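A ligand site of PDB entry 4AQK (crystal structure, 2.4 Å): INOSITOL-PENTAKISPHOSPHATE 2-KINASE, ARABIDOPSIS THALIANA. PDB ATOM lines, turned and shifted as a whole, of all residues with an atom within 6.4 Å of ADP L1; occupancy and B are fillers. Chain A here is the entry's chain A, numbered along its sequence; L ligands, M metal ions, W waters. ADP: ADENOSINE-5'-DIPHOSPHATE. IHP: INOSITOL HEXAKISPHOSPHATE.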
ATOM      1  N   ARG A  21     -17.613  26.288  28.005  1.00  0.00           N
ATOM      2  CA  ARG A  21     -16.319  25.649  27.942  1.00  0.00           C
ATOM      3  C   ARG A  21     -15.845  25.545  26.498  1.00  0.00           C
ATOM      4  O   ARG A  21     -14.729  25.961  26.159  1.00  0.00           O
ATOM      5  CB  ARG A  21     -16.422  24.266  28.584  1.00  0.00           C
ATOM      6  CG  ARG A  21     -15.189  23.410  28.468  1.00  0.00           C
ATOM      7  CD  ARG A  21     -13.964  24.120  29.033  1.00  0.00           C
ATOM      8  NE  ARG A  21     -13.180  23.178  29.823  1.00  0.00           N
ATOM      9  CZ  ARG A  21     -12.964  23.297  31.124  1.00  0.00           C
ATOM     10  NH1 ARG A  21     -13.449  24.329  31.804  1.00  0.00           N
ATOM     11  NH2 ARG A  21     -12.243  22.388  31.739  1.00  0.00           N
ATOM     12  N   GLY A  22     -16.704  24.973  25.645  1.00  0.00           N
ATOM     13  CA  GLY A  22     -16.437  24.822  24.227  1.00  0.00           C
ATOM     14  C   GLY A  22     -17.488  23.969  23.543  1.00  0.00           C
ATOM     15  O   GLY A  22     -18.419  23.462  24.183  1.00  0.00           O
ATOM     16  N   GLU A  23     -17.333  23.812  22.233  1.00  0.00           N
ATOM     17  CA  GLU A  23     -18.214  22.960  21.441  1.00  0.00           C
ATOM     18  C   GLU A  23     -17.518  22.448  20.194  1.00  0.00           C
ATOM     19  O   GLU A  23     -16.507  23.005  19.746  1.00  0.00           O
ATOM     20  CB  GLU A  23     -19.506  23.695  21.057  1.00  0.00           C
ATOM     21  CG  GLU A  23     -19.346  24.835  20.067  1.00  0.00           C
ATOM     22  CD  GLU A  23     -20.650  25.546  19.806  1.00  0.00           C
ATOM     23  OE1 GLU A  23     -21.509  24.990  19.101  1.00  0.00           O
ATOM     24  OE2 GLU A  23     -20.844  26.654  20.329  1.00  0.00           O
ATOM     25  N   GLY A  24     -18.053  21.364  19.641  1.00  0.00           N
ATOM     26  CA  GLY A  24     -17.677  20.900  18.310  1.00  0.00           C
ATOM     27  C   GLY A  24     -18.873  21.073  17.397  1.00  0.00           C
ATOM     28  O   GLY A  24     -19.533  22.108  17.423  1.00  0.00           O
ATOM     29  N   GLY A  25     -19.158  20.044  16.607  1.00  0.00           N
ATOM     30  CA  GLY A  25     -20.270  20.098  15.666  1.00  0.00           C
ATOM     31  C   GLY A  25     -21.533  19.411  16.172  1.00  0.00           C
ATOM     32  O   GLY A  25     -22.639  19.752  15.733  1.00  0.00           O
ATOM     33  N   ALA A  26     -21.378  18.460  17.075  1.00  0.00           N
ATOM     34  CA  ALA A  26     -22.509  17.685  17.583  1.00  0.00           C
ATOM     35  C   ALA A  26     -22.889  18.011  19.026  1.00  0.00           C
ATOM     36  O   ALA A  26     -24.031  17.796  19.435  1.00  0.00           O
ATOM     37  CB  ALA A  26     -22.226  16.188  17.436  1.00  0.00           C
ATOM     38  N   ASN A  27     -21.944  18.530  19.791  1.00  0.00           N
ATOM     39  CA  ASN A  27     -22.157  18.741  21.216  1.00  0.00           C
ATOM     40  C   ASN A  27     -21.740  20.102  21.742  1.00  0.00           C
ATOM     41  O   ASN A  27     -20.802  20.731  21.229  1.00  0.00           O
ATOM     42  CB  ASN A  27     -21.456  17.660  22.038  1.00  0.00           C
ATOM     43  CG  ASN A  27     -22.094  16.305  21.861  1.00  0.00           C
ATOM     44  OD1 ASN A  27     -21.508  15.398  21.261  1.00  0.00           O
ATOM     45  ND2 ASN A  27     -23.305  16.144  22.365  1.00  0.00           N
ATOM     46  N   LEU A  28     -22.451  20.536  22.782  1.00  0.00           N
ATOM     47  CA  LEU A  28     -22.100  21.710  23.564  1.00  0.00           C
ATOM     48  C   LEU A  28     -21.566  21.207  24.903  1.00  0.00           C
ATOM     49  O   LEU A  28     -22.121  20.285  25.516  1.00  0.00           O
ATOM     50  CB  LEU A  28     -23.334  22.595  23.768  1.00  0.00           C
ATOM     51  CG  LEU A  28     -23.131  24.064  24.138  1.00  0.00           C
ATOM     52  CD1 LEU A  28     -22.321  24.820  23.076  1.00  0.00           C
ATOM     53  CD2 LEU A  28     -24.469  24.745  24.328  1.00  0.00           C
ATOM     54  N   VAL A  29     -20.467  21.818  25.351  1.00  0.00           N
ATOM     55  CA  VAL A  29     -19.838  21.444  26.614  1.00  0.00           C
ATOM     56  C   VAL A  29     -19.747  22.645  27.549  1.00  0.00           C
ATOM     57  O   VAL A  29     -19.191  23.685  27.198  1.00  0.00           O
ATOM     58  CB  VAL A  29     -18.441  20.806  26.393  1.00  0.00           C
ATOM     59  CG1 VAL A  29     -17.712  20.607  27.729  1.00  0.00           C
ATOM     60  CG2 VAL A  29     -18.568  19.485  25.659  1.00  0.00           C
ATOM     61  N   VAL A  43     -17.854  18.546  33.926  1.00  0.00           N
ATOM     62  CA  VAL A  43     -18.396  19.229  32.739  1.00  0.00           C
ATOM     63  C   VAL A  43     -19.640  18.503  32.240  1.00  0.00           C
ATOM     64  O   VAL A  43     -19.840  17.321  32.516  1.00  0.00           O
ATOM     65  CB  VAL A  43     -17.375  19.341  31.583  1.00  0.00           C
ATOM     66  CG1 VAL A  43     -16.195  20.229  31.978  1.00  0.00           C
ATOM     67  CG2 VAL A  43     -16.904  17.960  31.112  1.00  0.00           C
ATOM     68  N   ARG A  45     -22.005  17.532  28.790  1.00  0.00           N
ATOM     69  CA  ARG A  45     -22.036  17.378  27.336  1.00  0.00           C
ATOM     70  C   ARG A  45     -23.489  17.326  26.874  1.00  0.00           C
ATOM     71  O   ARG A  45     -24.246  16.446  27.288  1.00  0.00           O
ATOM     72  CB  ARG A  45     -21.284  16.117  26.903  1.00  0.00           C
ATOM     73  CG  ARG A  45     -20.808  16.117  25.451  1.00  0.00           C
ATOM     74  CD  ARG A  45     -19.752  15.043  25.233  1.00  0.00           C
ATOM     75  NE  ARG A  45     -19.277  14.975  23.841  1.00  0.00           N
ATOM     76  CZ  ARG A  45     -19.501  13.960  23.008  1.00  0.00           C
ATOM     77  NH1 ARG A  45     -20.211  12.906  23.403  1.00  0.00           N
ATOM     78  NH2 ARG A  45     -19.015  13.999  21.781  1.00  0.00           N
ATOM     79  N   LYS A  48     -26.444  18.858  20.256  1.00  0.00           N
ATOM     80  CA  LYS A  48     -27.023  19.893  19.423  1.00  0.00           C
ATOM     81  C   LYS A  48     -27.908  19.293  18.333  1.00  0.00           C
ATOM     82  O   LYS A  48     -27.846  18.109  18.039  1.00  0.00           O
ATOM     83  CB  LYS A  48     -25.920  20.753  18.799  1.00  0.00           C
ATOM     84  CG  LYS A  48     -25.048  21.485  19.817  1.00  0.00           C
ATOM     85  CD  LYS A  48     -24.243  22.593  19.168  1.00  0.00           C
ATOM     86  CE  LYS A  48     -22.994  22.071  18.496  1.00  0.00           C
ATOM     87  NZ  LYS A  48     -22.400  23.101  17.598  1.00  0.00           N
ATOM     88  N   ARG A 135     -21.274  29.056  14.522  1.00  0.00           N
ATOM     89  CA  ARG A 135     -21.819  27.954  15.315  1.00  0.00           C
ATOM     90  C   ARG A 135     -23.302  28.171  15.614  1.00  0.00           C
ATOM     91  O   ARG A 135     -24.104  27.258  15.446  1.00  0.00           O
ATOM     92  CB  ARG A 135     -21.049  27.798  16.634  1.00  0.00           C
ATOM     93  CG  ARG A 135     -19.670  27.166  16.514  1.00  0.00           C
ATOM     94  CD  ARG A 135     -19.700  25.776  15.894  1.00  0.00           C
ATOM     95  NE  ARG A 135     -18.489  25.025  16.205  1.00  0.00           N
ATOM     96  CZ  ARG A 135     -18.100  23.905  15.606  1.00  0.00           C
ATOM     97  NH1 ARG A 135     -18.823  23.369  14.628  1.00  0.00           N
ATOM     98  NH2 ARG A 135     -16.973  23.320  15.982  1.00  0.00           N
ATOM     99  N   LEU A 151     -19.254  14.459  32.816  1.00  0.00           N
ATOM    100  CA  LEU A 151     -17.910  13.921  32.656  1.00  0.00           C
ATOM    101  C   LEU A 151     -16.947  14.644  33.579  1.00  0.00           C
ATOM    102  O   LEU A 151     -17.143  15.827  33.896  1.00  0.00           O
ATOM    103  CB  LEU A 151     -17.428  14.082  31.205  1.00  0.00           C
ATOM    104  CG  LEU A 151     -18.287  13.592  30.032  1.00  0.00           C
ATOM    105  CD1 LEU A 151     -18.008  14.431  28.813  1.00  0.00           C
ATOM    106  CD2 LEU A 151     -18.031  12.124  29.747  1.00  0.00           C
ATOM    107  N   ASN A 152     -15.909  13.944  34.011  1.00  0.00           N
ATOM    108  CA  ASN A 152     -14.835  14.567  34.758  1.00  0.00           C
ATOM    109  C   ASN A 152     -14.158  15.607  33.903  1.00  0.00           C
ATOM    110  O   ASN A 152     -13.734  15.329  32.784  1.00  0.00           O
ATOM    111  CB  ASN A 152     -13.813  13.521  35.222  1.00  0.00           C
ATOM    112  CG  ASN A 152     -14.421  12.483  36.137  1.00  0.00           C
ATOM    113  OD1 ASN A 152     -14.246  11.276  35.923  1.00  0.00           O
ATOM    114  ND2 ASN A 152     -15.138  12.934  37.160  1.00  0.00           N
ATOM    115  N   ASP A 153     -14.077  16.825  34.436  1.00  0.00           N
ATOM    116  CA  ASP A 153     -13.394  17.920  33.766  1.00  0.00           C
ATOM    117  C   ASP A 153     -11.906  17.618  33.742  1.00  0.00           C
ATOM    118  O   ASP A 153     -11.226  17.671  34.769  1.00  0.00           O
ATOM    119  CB  ASP A 153     -13.653  19.250  34.493  1.00  0.00           C
ATOM    120  CG  ASP A 153     -12.971  20.423  33.826  1.00  0.00           C
ATOM    121  OD1 ASP A 153     -12.057  20.211  32.991  1.00  0.00           O
ATOM    122  OD2 ASP A 153     -13.336  21.571  34.132  1.00  0.00           O
ATOM    123  N   HIS A 154     -11.404  17.322  32.545  1.00  0.00           N
ATOM    124  CA  HIS A 154     -10.028  16.878  32.396  1.00  0.00           C
ATOM    125  C   HIS A 154      -8.995  18.008  32.510  1.00  0.00           C
ATOM    126  O   HIS A 154      -7.789  17.746  32.462  1.00  0.00           O
ATOM    127  CB  HIS A 154      -9.861  16.090  31.090  1.00  0.00           C
ATOM    128  CG  HIS A 154     -10.693  14.847  31.027  1.00  0.00           C
ATOM    129  ND1 HIS A 154     -10.624  13.849  31.981  1.00  0.00           N
ATOM    130  CD2 HIS A 154     -11.614  14.437  30.124  1.00  0.00           C
ATOM    131  CE1 HIS A 154     -11.468  12.886  31.666  1.00  0.00           C
ATOM    132  NE2 HIS A 154     -12.085  13.219  30.547  1.00  0.00           N
ATOM    133  N   SER A 155      -9.458  19.244  32.672  1.00  0.00           N
ATOM    134  CA  SER A 155      -8.551  20.357  32.956  1.00  0.00           C
ATOM    135  C   SER A 155      -8.282  20.494  34.458  1.00  0.00           C
ATOM    136  O   SER A 155      -7.514  21.364  34.884  1.00  0.00           O
ATOM    137  CB  SER A 155      -9.099  21.663  32.372  1.00  0.00           C
ATOM    138  OG  SER A 155     -10.263  22.061  33.062  1.00  0.00           O
ATOM    139  N   GLU A 171      -5.348  20.044  25.010  1.00  0.00           N
ATOM    140  CA  GLU A 171      -6.204  19.283  24.110  1.00  0.00           C
ATOM    141  C   GLU A 171      -5.596  19.191  22.706  1.00  0.00           C
ATOM    142  O   GLU A 171      -5.148  20.195  22.153  1.00  0.00           O
ATOM    143  CB  GLU A 171      -7.592  19.907  24.025  1.00  0.00           C
ATOM    144  CG  GLU A 171      -8.541  19.110  23.129  1.00  0.00           C
ATOM    145  CD  GLU A 171      -9.814  19.863  22.755  1.00  0.00           C
ATOM    146  OE1 GLU A 171      -9.779  21.117  22.667  1.00  0.00           O
ATOM    147  OE2 GLU A 171     -10.833  19.181  22.537  1.00  0.00           O
ATOM    148  N   LYS A 173      -6.449  17.507  18.773  1.00  0.00           N
ATOM    149  CA  LYS A 173      -7.301  16.824  17.785  1.00  0.00           C
ATOM    150  C   LYS A 173      -6.403  16.355  16.648  1.00  0.00           C
ATOM    151  O   LYS A 173      -6.083  17.116  15.726  1.00  0.00           O
ATOM    152  CB  LYS A 173      -8.373  17.763  17.255  1.00  0.00           C
ATOM    153  CG  LYS A 173      -9.592  17.074  16.702  1.00  0.00           C
ATOM    154  CD  LYS A 173     -10.414  18.043  15.878  1.00  0.00           C
ATOM    155  CE  LYS A 173     -11.899  17.868  16.124  1.00  0.00           C
ATOM    156  NZ  LYS A 173     -12.433  16.668  15.441  1.00  0.00           N
ATOM    157  N   ARG A 246      -5.529  23.096  21.865  1.00  0.00           N
ATOM    158  CA  ARG A 246      -6.006  23.997  22.914  1.00  0.00           C
ATOM    159  C   ARG A 246      -5.214  23.817  24.216  1.00  0.00           C
ATOM    160  O   ARG A 246      -4.841  22.703  24.579  1.00  0.00           O
ATOM    161  CB  ARG A 246      -7.497  23.807  23.179  1.00  0.00           C
ATOM    162  CG  ARG A 246      -8.348  24.297  22.033  1.00  0.00           C
ATOM    163  CD  ARG A 246      -9.825  24.284  22.335  1.00  0.00           C
ATOM    164  NE  ARG A 246     -10.563  24.575  21.108  1.00  0.00           N
ATOM    165  CZ  ARG A 246     -11.219  23.686  20.387  1.00  0.00           C
ATOM    166  NH1 ARG A 246     -11.271  22.410  20.764  1.00  0.00           N
ATOM    167  NH2 ARG A 246     -11.826  24.069  19.279  1.00  0.00           N
ATOM    168  N   PHE A 248      -5.409  24.926  28.403  1.00  0.00           N
ATOM    169  CA  PHE A 248      -6.217  25.459  29.493  1.00  0.00           C
ATOM    170  C   PHE A 248      -5.392  25.568  30.793  1.00  0.00           C
ATOM    171  O   PHE A 248      -4.649  24.648  31.131  1.00  0.00           O
ATOM    172  CB  PHE A 248      -7.419  24.565  29.757  1.00  0.00           C
ATOM    173  CG  PHE A 248      -8.355  24.404  28.582  1.00  0.00           C
ATOM    174  CD1 PHE A 248      -8.137  23.414  27.631  1.00  0.00           C
ATOM    175  CD2 PHE A 248      -9.463  25.235  28.446  1.00  0.00           C
ATOM    176  CE1 PHE A 248      -9.004  23.262  26.547  1.00  0.00           C
ATOM    177  CE2 PHE A 248     -10.342  25.088  27.373  1.00  0.00           C
ATOM    178  CZ  PHE A 248     -10.110  24.096  26.420  1.00  0.00           C
ATOM    179  N   ASP A 373     -11.730  11.551  14.357  1.00  0.00           N
ATOM    180  CA  ASP A 373     -12.395  12.777  14.783  1.00  0.00           C
ATOM    181  C   ASP A 373     -12.418  13.018  16.304  1.00  0.00           C
ATOM    182  O   ASP A 373     -13.015  13.984  16.784  1.00  0.00           O
ATOM    183  CB  ASP A 373     -13.815  12.798  14.229  1.00  0.00           C
ATOM    184  CG  ASP A 373     -14.461  14.155  14.311  1.00  0.00           C
ATOM    185  OD1 ASP A 373     -13.853  15.126  13.787  1.00  0.00           O
ATOM    186  OD2 ASP A 373     -15.574  14.256  14.874  1.00  0.00           O
ATOM    187  N   SER A 375     -10.581  13.539  20.272  1.00  0.00           N
ATOM    188  CA  SER A 375      -9.564  14.406  20.836  1.00  0.00           C
ATOM    189  C   SER A 375      -8.845  13.749  22.014  1.00  0.00           C
ATOM    190  O   SER A 375      -9.348  12.801  22.614  1.00  0.00           O
ATOM    191  CB  SER A 375     -10.167  15.747  21.256  1.00  0.00           C
ATOM    192  OG  SER A 375     -10.930  16.314  20.202  1.00  0.00           O
ATOM    193  N   MET A 377      -6.917  14.767  25.662  1.00  0.00           N
ATOM    194  CA  MET A 377      -6.624  15.760  26.697  1.00  0.00           C
ATOM    195  C   MET A 377      -5.527  15.244  27.616  1.00  0.00           C
ATOM    196  O   MET A 377      -5.630  14.141  28.157  1.00  0.00           O
ATOM    197  CB  MET A 377      -7.876  16.143  27.480  1.00  0.00           C
ATOM    198  CG  MET A 377      -8.961  16.787  26.629  1.00  0.00           C
ATOM    199  SD  MET A 377     -10.010  17.983  27.503  1.00  0.00           S
ATOM    200  CE  MET A 377      -8.844  19.297  27.864  1.00  0.00           C
ATOM    201  N   ILE A 411     -11.420  12.074  24.493  1.00  0.00           N
ATOM    202  CA  ILE A 411     -12.755  12.696  24.507  1.00  0.00           C
ATOM    203  C   ILE A 411     -13.346  12.747  23.108  1.00  0.00           C
ATOM    204  O   ILE A 411     -12.651  12.468  22.121  1.00  0.00           O
ATOM    205  CB  ILE A 411     -12.738  14.111  25.110  1.00  0.00           C
ATOM    206  CG1 ILE A 411     -11.821  15.028  24.288  1.00  0.00           C
ATOM    207  CG2 ILE A 411     -12.307  14.085  26.571  1.00  0.00           C
ATOM    208  CD1 ILE A 411     -12.216  16.491  24.332  1.00  0.00           C
ATOM    209  N   ASP A 412     -14.624  13.121  23.019  1.00  0.00           N
ATOM    210  CA  ASP A 412     -15.308  13.303  21.745  1.00  0.00           C
ATOM    211  C   ASP A 412     -15.271  12.008  20.927  1.00  0.00           C
ATOM    212  O   ASP A 412     -14.755  11.975  19.809  1.00  0.00           O
ATOM    213  CB  ASP A 412     -14.676  14.467  20.973  1.00  0.00           C
ATOM    214  CG  ASP A 412     -15.381  14.782  19.662  1.00  0.00           C
ATOM    215  OD1 ASP A 412     -16.578  14.439  19.518  1.00  0.00           O
ATOM    216  OD2 ASP A 412     -14.729  15.392  18.785  1.00  0.00           O
ATOM    217  N   LEU A 413     -15.813  10.933  21.509  1.00  0.00           N
ATOM    218  CA  LEU A 413     -15.872   9.652  20.830  1.00  0.00           C
ATOM    219  C   LEU A 413     -17.300   9.369  20.355  1.00  0.00           C
ATOM    220  O   LEU A 413     -17.944   8.405  20.797  1.00  0.00           O
ATOM    221  CB  LEU A 413     -15.349   8.537  21.753  1.00  0.00           C
ATOM    222  CG  LEU A 413     -13.860   8.538  22.138  1.00  0.00           C
ATOM    223  CD1 LEU A 413     -13.605   7.527  23.251  1.00  0.00           C
ATOM    224  CD2 LEU A 413     -12.931   8.267  20.948  1.00  0.00           C
ATOM    225  N   SER A 414     -17.770  10.202  19.432  1.00  0.00           N
ATOM    226  CA  SER A 414     -19.148  10.140  18.945  1.00  0.00           C
ATOM    227  C   SER A 414     -19.423   8.988  17.958  1.00  0.00           C
ATOM    228  O   SER A 414     -18.578   8.665  17.118  1.00  0.00           O
ATOM    229  CB  SER A 414     -19.551  11.473  18.292  1.00  0.00           C
ATOM    230  OG  SER A 414     -19.280  12.570  19.147  1.00  0.00           O
HETATM  231  PB  ADP L   1     -18.461  17.664  19.889  1.00  0.00           P
HETATM  232  O1B ADP L   1     -19.486  18.672  19.441  1.00  0.00           O
HETATM  233  O2B ADP L   1     -17.228  17.653  19.017  1.00  0.00           O
HETATM  234  O3B ADP L   1     -19.046  16.300  20.178  1.00  0.00           O
HETATM  235  PA  ADP L   1     -16.627  17.615  22.097  1.00  0.00           P
HETATM  236  O1A ADP L   1     -17.030  16.354  22.819  1.00  0.00           O
HETATM  237  O2A ADP L   1     -15.442  17.604  21.160  1.00  0.00           O
HETATM  238  O3A ADP L   1     -17.941  18.191  21.329  1.00  0.00           O
HETATM  239  O5' ADP L   1     -16.348  18.766  23.193  1.00  0.00           O
HETATM  240  C5' ADP L   1     -16.236  20.131  22.821  1.00  0.00           C
HETATM  241  C4' ADP L   1     -15.089  20.832  23.531  1.00  0.00           C
HETATM  242  O4' ADP L   1     -15.266  20.824  24.957  1.00  0.00           O
HETATM  243  C3' ADP L   1     -13.760  20.153  23.254  1.00  0.00           C
HETATM  244  O3' ADP L   1     -13.033  20.866  22.251  1.00  0.00           O
HETATM  245  C2' ADP L   1     -13.026  20.116  24.590  1.00  0.00           C
HETATM  246  O2' ADP L   1     -12.025  21.125  24.683  1.00  0.00           O
HETATM  247  C1' ADP L   1     -14.079  20.401  25.640  1.00  0.00           C
HETATM  248  N9  ADP L   1     -14.344  19.178  26.445  1.00  0.00           N
HETATM  249  C8  ADP L   1     -15.181  18.180  26.120  1.00  0.00           C
HETATM  250  N7  ADP L   1     -15.216  17.215  27.076  1.00  0.00           N
HETATM  251  C5  ADP L   1     -14.380  17.595  28.055  1.00  0.00           C
HETATM  252  C6  ADP L   1     -13.939  17.051  29.367  1.00  0.00           C
HETATM  253  N6  ADP L   1     -14.397  15.864  29.830  1.00  0.00           N
HETATM  254  N1  ADP L   1     -13.044  17.768  30.077  1.00  0.00           N
HETATM  255  C2  ADP L   1     -12.559  18.956  29.640  1.00  0.00           C
HETATM  256  N3  ADP L   1     -12.911  19.507  28.458  1.00  0.00           N
HETATM  257  C4  ADP L   1     -13.807  18.899  27.639  1.00  0.00           C
HETATM  258  C1  IHP L   2     -16.352  16.021  11.669  1.00  0.00           C
HETATM  259  C2  IHP L   2     -17.360  16.877  12.437  1.00  0.00           C
HETATM  260  C3  IHP L   2     -16.688  17.969  13.262  1.00  0.00           C
HETATM  261  C4  IHP L   2     -15.780  18.826  12.367  1.00  0.00           C
HETATM  262  C5  IHP L   2     -14.738  17.986  11.607  1.00  0.00           C
HETATM  263  C6  IHP L   2     -15.392  16.848  10.807  1.00  0.00           C
HETATM  264  O11 IHP L   2     -17.063  15.116  10.824  1.00  0.00           O
HETATM  265  P1  IHP L   2     -16.824  13.516  10.806  1.00  0.00           P
HETATM  266  O21 IHP L   2     -15.919  13.307   9.630  1.00  0.00           O
HETATM  267  O31 IHP L   2     -16.202  13.146  12.114  1.00  0.00           O
HETATM  268  O41 IHP L   2     -18.231  12.963  10.665  1.00  0.00           O
HETATM  269  O12 IHP L   2     -18.069  16.012  13.319  1.00  0.00           O
HETATM  270  P2  IHP L   2     -19.654  16.097  13.575  1.00  0.00           P
HETATM  271  O22 IHP L   2     -19.793  16.979  14.781  1.00  0.00           O
HETATM  272  O32 IHP L   2     -20.283  16.699  12.341  1.00  0.00           O
HETATM  273  O42 IHP L   2     -19.989  14.645  13.837  1.00  0.00           O
HETATM  274  O13 IHP L   2     -15.953  17.385  14.340  1.00  0.00           O
HETATM  275  P3  IHP L   2     -16.380  17.513  15.906  1.00  0.00           P
HETATM  276  O23 IHP L   2     -15.541  18.669  16.422  1.00  0.00           O
HETATM  277  O33 IHP L   2     -17.864  17.754  15.932  1.00  0.00           O
HETATM  278  O43 IHP L   2     -16.022  16.193  16.543  1.00  0.00           O
HETATM  279  O14 IHP L   2     -15.119  19.809  13.149  1.00  0.00           O
HETATM  280  P4  IHP L   2     -15.572  21.359  13.273  1.00  0.00           P
HETATM  281  O24 IHP L   2     -17.078  21.343  13.417  1.00  0.00           O
HETATM  282  O34 IHP L   2     -15.094  22.026  12.018  1.00  0.00           O
HETATM  283  O44 IHP L   2     -14.814  21.791  14.505  1.00  0.00           O
HETATM  284  O15 IHP L   2     -14.016  18.821  10.711  1.00  0.00           O
HETATM  285  P5  IHP L   2     -12.507  19.351  10.914  1.00  0.00           P
HETATM  286  O25 IHP L   2     -11.844  19.173   9.575  1.00  0.00           O
HETATM  287  O35 IHP L   2     -12.693  20.803  11.287  1.00  0.00           O
HETATM  288  O45 IHP L   2     -11.883  18.475  11.971  1.00  0.00           O
HETATM  289  O16 IHP L   2     -14.390  15.964  10.317  1.00  0.00           O
HETATM  290  P6  IHP L   2     -13.913  15.893   8.771  1.00  0.00           P
HETATM  291  O26 IHP L   2     -12.587  15.181   8.796  1.00  0.00           O
HETATM  292  O36 IHP L   2     -15.023  15.098   8.157  1.00  0.00           O
HETATM  293  O46 IHP L   2     -13.786  17.331   8.301  1.00  0.00           O
HETATM  294 MG    MG M   1     -18.393  14.725  17.565  1.00  0.00          MG
HETATM  295  O   HOH W   1     -14.310  18.986  19.350  1.00  0.00           O
HETATM  296  O   HOH W   2     -16.467  14.576  25.397  1.00  0.00           O
HETATM  297  O   HOH W   3     -14.610  23.732  21.453  1.00  0.00           O
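SD of Met 377 lies close to N3 of ADP L1 (3.4 Å).
OD1 of Asp 412 lies close to O3B of ADP L1 (3.2 Å).
Merely in contact with ADP L1: Arg 21, Gly 22, Glu 23, Val 29, Val 43, Leu 151, Asp 153, Phe 248, Ile 411 and Ser 414.
Hydrophobic or aromatic side chains within 4 Å of ADP L1: Val 29, Val 43, Leu 151, His 154, Phe 248, Met 377 and Ile 411.
An oxygen (O1B) of ADP L1 sits close to the backbone carbonyl oxygen (O) of Asn 27, at 3.0 Å.
O of Asn 152 is in hydrogen-bond range of N6 of ADP L1, at 3.1 Å.
The side-chain amino group (NZ) of Lys 173 lies within salt-bridge range of an oxygen (O43) of IHP L2 (3.8 Å).
An oxygen (O1B) of ADP L1 lies within hydrogen-bond range of the backbone NH (N) of Gly 24 (3.1 Å).
An oxygen (O3B) of ADP L1 is in salt-bridge range of the guanidinium group of Arg 45, 2.8 Å away.
OD1 of Asn 27 sits close to O3B of ADP L1, at 2.8 Å.
An oxygen (O1B) of ADP L1 sits at hydrogen-bond distance from the backbone NH of Ala 26, 3.0 Å away.
N of Ala 26 lies within hydrogen-bond range of O22 of IHP L2, at 3.2 Å.
The guanidinium group (NH1) of Arg 246 lies within hydrogen-bond range of an oxygen (O3') of ADP L1 (2.8 Å).
The backbone NH (N) of His 154 is in hydrogen-bond range of a nitrogen (N1) of ADP L1 (3.0 Å).
An oxygen (O43) of IHP L2 sits close to the side-chain carboxylate of Asp 412 (2.7 Å).
The side-chain carboxylate (OD2) of Asp 373 sits close to an oxygen (O43) of IHP L2 (2.6 Å).
OE2 of Glu 171 is in hydrogen-bond range of O3' of ADP L1, at 2.8 Å.
The backbone NH of Gly 25 sits at hydrogen-bond distance from an oxygen (O1B) of ADP L1, at 3.2 Å.
N of Asn 27 lies within hydrogen-bond range of O1B of ADP L1, at 2.5 Å.
NH1 of Arg 135 is in salt-bridge range of O24 of IHP L2 (2.9 Å).
The backbone NH (N) of Gly 25 lies within hydrogen-bond range of an oxygen (O33) of IHP L2 (2.7 Å).
The backbone carbonyl oxygen (O) of Asn 152 is in hydrogen-bond range of a ring nitrogen (NE2) of His 154.
OG of Ser 414 lies within hydrogen-bond range of NH2 of Arg 45.
O of Val 29 sits at hydrogen-bond distance from N of Arg 21, 3.1 Å away.
The side-chain hydroxyl of Ser 155 is in hydrogen-bond range of the side-chain carboxylate of Asp 153 (2.6 Å).
O of Ser 375 lies within hydrogen-bond range of N of Ile 411 (2.9 Å).
The side-chain hydroxyl (OG) of Ser 414 lies within hydrogen-bond range of the side-chain carboxylate (OD1) of Asp 412 (3.3 Å).
The backbone carbonyl oxygen (O) of Gly 22 is in hydrogen-bond range of the backbone NH (N) of Val 29 (2.9 Å).
The backbone carbonyl oxygen (O) of Gly 24 is in hydrogen-bond range of the side-chain amino group (NZ) of Lys 48 (3.0 Å).
Water W1 bridges an oxygen (O2A) of ADP L1 (2.5 Å) and an oxygen (O23) of IHP L2 (3.2 Å).
Water W2 lies within hydrogen-bond range of an oxygen (O1A) of ADP L1 (3.2 Å), the guanidinium group (NE) of Arg 45 (3.2 Å) and the backbone NH (N) of Asp 412 (3.3 Å).
Water W3 lies within hydrogen-bond range of the backbone carbonyl oxygen (O) of Glu 23 and an oxygen (O3') of ADP L1.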
